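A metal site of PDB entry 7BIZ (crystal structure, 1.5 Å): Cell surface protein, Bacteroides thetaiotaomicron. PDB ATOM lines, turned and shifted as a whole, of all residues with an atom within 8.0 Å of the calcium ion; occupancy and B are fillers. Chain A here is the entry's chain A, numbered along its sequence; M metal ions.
N of Asp 324 sits at hydrogen-bond distance from SD of Met 313, at 3.4 Å.
The side-chain carboxylate (OD2) of Asp 315 lies within hydrogen-bond range of the backbone NH (N) of Gly 320 (2.8 Å).
The backbone NH of Ile 316 sits at hydrogen-bond distance from the side-chain carboxylate of Asp 324, at 3.2 Å.
OD2 of Asp 463 lies within hydrogen-bond range of N of Asp 315.
N of Asp 323 lies within hydrogen-bond range of SD of Met 313.
OD1 of Asp 315 sits close to N of Gly 318 (3.5 Å).
The calcium ion is bound by the side-chain carboxylate of Asp 315, the side-chain carboxylate of Asp 324, the side-chain carboxylate of Asp 323, the side-chain amide oxygen of Asn 317, the backbone carbonyl oxygen of Leu 321 and the side-chain amide oxygen of Asn 319.
The calcium ion has six donor atoms within binding distance.
The nearest printed residue that does not touch the calcium ion is Gly 318 (4.5 Å).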
ATOM      1  N   GLN A 115      35.041  22.499  -9.865  1.00  0.00           N
ATOM      2  CA  GLN A 115      34.207  21.656 -10.708  1.00  0.00           C
ATOM      3  C   GLN A 115      34.185  22.159 -12.150  1.00  0.00           C
ATOM      4  O   GLN A 115      34.200  23.369 -12.401  1.00  0.00           O
ATOM      5  CB  GLN A 115      32.792  21.609 -10.136  1.00  0.00           C
ATOM      6  CG  GLN A 115      32.729  20.857  -8.793  1.00  0.00           C
ATOM      7  CD  GLN A 115      31.334  20.851  -8.191  1.00  0.00           C
ATOM      8  OE1 GLN A 115      30.384  20.415  -8.837  1.00  0.00           O
ATOM      9  NE2 GLN A 115      31.197  21.332  -6.951  1.00  0.00           N
ATOM     10  N   TYR A 121      20.692  20.702 -12.985  1.00  0.00           N
ATOM     11  CA  TYR A 121      19.755  19.684 -12.536  1.00  0.00           C
ATOM     12  C   TYR A 121      18.571  20.342 -11.848  1.00  0.00           C
ATOM     13  O   TYR A 121      18.744  21.265 -11.051  1.00  0.00           O
ATOM     14  CB  TYR A 121      20.420  18.687 -11.550  1.00  0.00           C
ATOM     15  CG  TYR A 121      21.629  18.047 -12.155  1.00  0.00           C
ATOM     16  CD1 TYR A 121      22.848  18.673 -12.094  1.00  0.00           C
ATOM     17  CD2 TYR A 121      21.530  16.830 -12.816  1.00  0.00           C
ATOM     18  CE1 TYR A 121      23.995  18.092 -12.692  1.00  0.00           C
ATOM     19  CE2 TYR A 121      22.653  16.247 -13.396  1.00  0.00           C
ATOM     20  CZ  TYR A 121      23.872  16.891 -13.318  1.00  0.00           C
ATOM     21  OH  TYR A 121      25.014  16.354 -13.886  1.00  0.00           O
ATOM     22  N   MET A 313      22.008  24.140  -1.102  1.00  0.00           N
ATOM     23  CA  MET A 313      21.871  23.275  -2.256  1.00  0.00           C
ATOM     24  C   MET A 313      21.203  21.981  -1.810  1.00  0.00           C
ATOM     25  O   MET A 313      21.573  21.414  -0.776  1.00  0.00           O
ATOM     26  CB  MET A 313      23.251  22.976  -2.872  1.00  0.00           C
ATOM     27  CG  MET A 313      23.217  21.946  -4.022  1.00  0.00           C
ATOM     28  SD  MET A 313      24.910  21.601  -4.613  1.00  0.00           S
ATOM     29  CE  MET A 313      25.358  23.119  -5.505  1.00  0.00           C
ATOM     30  N   GLN A 314      20.230  21.537  -2.602  1.00  0.00           N
ATOM     31  CA  GLN A 314      19.715  20.164  -2.537  1.00  0.00           C
ATOM     32  C   GLN A 314      20.517  19.270  -3.478  1.00  0.00           C
ATOM     33  O   GLN A 314      20.895  19.677  -4.575  1.00  0.00           O
ATOM     34  CB  GLN A 314      18.248  20.099  -2.935  1.00  0.00           C
ATOM     35  CG  GLN A 314      17.330  20.829  -1.929  1.00  0.00           C
ATOM     36  CD  GLN A 314      15.919  20.872  -2.424  1.00  0.00           C
ATOM     37  OE1 GLN A 314      15.668  21.200  -3.572  1.00  0.00           O
ATOM     38  NE2 GLN A 314      14.983  20.479  -1.557  1.00  0.00           N
ATOM     39  N   ASP A 315      20.696  18.001  -3.064  1.00  0.00           N
ATOM     40  CA  ASP A 315      21.390  17.009  -3.890  1.00  0.00           C
ATOM     41  C   ASP A 315      20.407  16.427  -4.920  1.00  0.00           C
ATOM     42  O   ASP A 315      20.001  15.261  -4.860  1.00  0.00           O
ATOM     43  CB  ASP A 315      22.008  15.939  -2.990  1.00  0.00           C
ATOM     44  CG  ASP A 315      22.795  14.894  -3.751  1.00  0.00           C
ATOM     45  OD1 ASP A 315      23.350  15.229  -4.820  1.00  0.00           O
ATOM     46  OD2 ASP A 315      22.838  13.723  -3.274  1.00  0.00           O
ATOM     47  N   ILE A 316      19.960  17.318  -5.829  1.00  0.00           N
ATOM     48  CA  ILE A 316      18.897  16.998  -6.774  1.00  0.00           C
ATOM     49  C   ILE A 316      19.213  15.711  -7.511  1.00  0.00           C
ATOM     50  O   ILE A 316      18.348  14.851  -7.692  1.00  0.00           O
ATOM     51  CB  ILE A 316      18.691  18.164  -7.757  1.00  0.00           C
ATOM     52  CG1 ILE A 316      18.292  19.414  -6.951  1.00  0.00           C
ATOM     53  CG2 ILE A 316      17.633  17.810  -8.797  1.00  0.00           C
ATOM     54  CD1 ILE A 316      18.082  20.644  -7.819  1.00  0.00           C
ATOM     55  N   ASN A 317      20.455  15.582  -7.996  1.00  0.00           N
ATOM     56  CA  ASN A 317      20.760  14.412  -8.801  1.00  0.00           C
ATOM     57  C   ASN A 317      21.184  13.193  -7.984  1.00  0.00           C
ATOM     58  O   ASN A 317      21.518  12.160  -8.577  1.00  0.00           O
ATOM     59  CB  ASN A 317      21.830  14.753  -9.843  1.00  0.00           C
ATOM     60  CG  ASN A 317      23.152  15.182  -9.241  1.00  0.00           C
ATOM     61  OD1 ASN A 317      23.449  14.946  -8.075  1.00  0.00           O
ATOM     62  ND2 ASN A 317      23.963  15.864 -10.064  1.00  0.00           N
ATOM     63  N   GLY A 318      21.145  13.272  -6.651  1.00  0.00           N
ATOM     64  CA  GLY A 318      21.209  12.074  -5.823  1.00  0.00           C
ATOM     65  C   GLY A 318      22.567  11.425  -5.679  1.00  0.00           C
ATOM     66  O   GLY A 318      22.656  10.293  -5.205  1.00  0.00           O
ATOM     67  N   ASN A 319      23.647  12.109  -6.071  1.00  0.00           N
ATOM     68  CA  ASN A 319      24.941  11.446  -6.109  1.00  0.00           C
ATOM     69  C   ASN A 319      25.809  11.742  -4.894  1.00  0.00           C
ATOM     70  O   ASN A 319      26.962  11.285  -4.850  1.00  0.00           O
ATOM     71  CB  ASN A 319      25.698  11.801  -7.408  1.00  0.00           C
ATOM     72  CG  ASN A 319      25.993  13.298  -7.532  1.00  0.00           C
ATOM     73  OD1 ASN A 319      25.755  14.102  -6.623  1.00  0.00           O
ATOM     74  ND2 ASN A 319      26.510  13.678  -8.713  1.00  0.00           N
ATOM     75  N   GLY A 320      25.290  12.467  -3.896  1.00  0.00           N
ATOM     76  CA  GLY A 320      26.071  12.781  -2.727  1.00  0.00           C
ATOM     77  C   GLY A 320      27.038  13.934  -2.880  1.00  0.00           C
ATOM     78  O   GLY A 320      27.669  14.337  -1.897  1.00  0.00           O
ATOM     79  N   LEU A 321      27.155  14.521  -4.086  1.00  0.00           N
ATOM     80  CA  LEU A 321      28.109  15.577  -4.363  1.00  0.00           C
ATOM     81  C   LEU A 321      27.409  16.916  -4.512  1.00  0.00           C
ATOM     82  O   LEU A 321      26.291  16.976  -5.036  1.00  0.00           O
ATOM     83  CB  LEU A 321      28.881  15.274  -5.651  1.00  0.00           C
ATOM     84  CG  LEU A 321      29.642  13.971  -5.584  1.00  0.00           C
ATOM     85  CD1 LEU A 321      30.221  13.655  -6.959  1.00  0.00           C
ATOM     86  CD2 LEU A 321      30.742  14.058  -4.513  1.00  0.00           C
ATOM     87  N   PRO A 322      28.069  18.016  -4.100  1.00  0.00           N
ATOM     88  CA  PRO A 322      27.474  19.356  -4.229  1.00  0.00           C
ATOM     89  C   PRO A 322      27.665  19.946  -5.616  1.00  0.00           C
ATOM     90  O   PRO A 322      28.332  20.945  -5.828  1.00  0.00           O
ATOM     91  CB  PRO A 322      28.213  20.158  -3.136  1.00  0.00           C
ATOM     92  CG  PRO A 322      29.632  19.537  -3.124  1.00  0.00           C
ATOM     93  CD  PRO A 322      29.347  18.042  -3.329  1.00  0.00           C
ATOM     94  N   ASP A 323      27.027  19.292  -6.599  1.00  0.00           N
ATOM     95  CA  ASP A 323      27.180  19.634  -8.008  1.00  0.00           C
ATOM     96  C   ASP A 323      25.848  20.006  -8.634  1.00  0.00           C
ATOM     97  O   ASP A 323      25.715  20.015  -9.870  1.00  0.00           O
ATOM     98  CB  ASP A 323      27.832  18.464  -8.758  1.00  0.00           C
ATOM     99  CG  ASP A 323      26.981  17.203  -8.759  1.00  0.00           C
ATOM    100  OD1 ASP A 323      25.956  17.108  -8.062  1.00  0.00           O
ATOM    101  OD2 ASP A 323      27.363  16.274  -9.510  1.00  0.00           O
ATOM    102  N   ASP A 324      24.862  20.322  -7.786  1.00  0.00           N
ATOM    103  CA  ASP A 324      23.541  20.692  -8.251  1.00  0.00           C
ATOM    104  C   ASP A 324      23.409  22.208  -8.272  1.00  0.00           C
ATOM    105  O   ASP A 324      24.335  22.902  -8.699  1.00  0.00           O
ATOM    106  CB  ASP A 324      22.488  20.009  -7.348  1.00  0.00           C
ATOM    107  CG  ASP A 324      22.752  18.521  -7.204  1.00  0.00           C
ATOM    108  OD1 ASP A 324      23.513  18.148  -6.301  1.00  0.00           O
ATOM    109  OD2 ASP A 324      22.237  17.754  -8.036  1.00  0.00           O
ATOM    110  N   GLU A 325      22.251  22.742  -7.873  1.00  0.00           N
ATOM    111  CA  GLU A 325      21.974  24.189  -7.939  1.00  0.00           C
ATOM    112  C   GLU A 325      22.192  24.867  -6.582  1.00  0.00           C
ATOM    113  O   GLU A 325      21.697  24.388  -5.561  1.00  0.00           O
ATOM    114  CB  GLU A 325      20.510  24.398  -8.391  1.00  0.00           C
ATOM    115  CG  GLU A 325      20.239  25.808  -8.912  1.00  0.00           C
ATOM    116  CD  GLU A 325      20.663  26.035 -10.374  1.00  0.00           C
ATOM    117  OE1 GLU A 325      21.055  25.070 -11.082  1.00  0.00           O
ATOM    118  OE2 GLU A 325      20.595  27.222 -10.815  1.00  0.00           O
ATOM    119  N   ASP A 463      20.835  19.995   1.534  1.00  0.00           N
ATOM    120  CA  ASP A 463      21.884  19.009   1.773  1.00  0.00           C
ATOM    121  C   ASP A 463      23.277  19.603   1.909  1.00  0.00           C
ATOM    122  O   ASP A 463      24.119  18.997   2.569  1.00  0.00           O
ATOM    123  CB  ASP A 463      21.916  17.982   0.627  1.00  0.00           C
ATOM    124  CG  ASP A 463      20.634  17.187   0.568  1.00  0.00           C
ATOM    125  OD1 ASP A 463      20.334  16.521   1.595  1.00  0.00           O
ATOM    126  OD2 ASP A 463      19.920  17.219  -0.469  1.00  0.00           O
ATOM    127  N   PHE A 464      23.546  20.761   1.311  1.00  0.00           N
ATOM    128  CA  PHE A 464      24.860  21.374   1.395  1.00  0.00           C
ATOM    129  C   PHE A 464      24.717  22.853   1.700  1.00  0.00           C
ATOM    130  O   PHE A 464      23.736  23.482   1.322  1.00  0.00           O
ATOM    131  CB  PHE A 464      25.639  21.238   0.065  1.00  0.00           C
ATOM    132  CG  PHE A 464      25.677  19.848  -0.500  1.00  0.00           C
ATOM    133  CD1 PHE A 464      26.620  18.933  -0.064  1.00  0.00           C
ATOM    134  CD2 PHE A 464      24.763  19.465  -1.487  1.00  0.00           C
ATOM    135  CE1 PHE A 464      26.678  17.629  -0.629  1.00  0.00           C
ATOM    136  CE2 PHE A 464      24.809  18.187  -2.032  1.00  0.00           C
ATOM    137  CZ  PHE A 464      25.756  17.264  -1.592  1.00  0.00           C
HETATM  138 CA    CA M   1      24.605  16.168  -6.455  1.00  0.00          CA
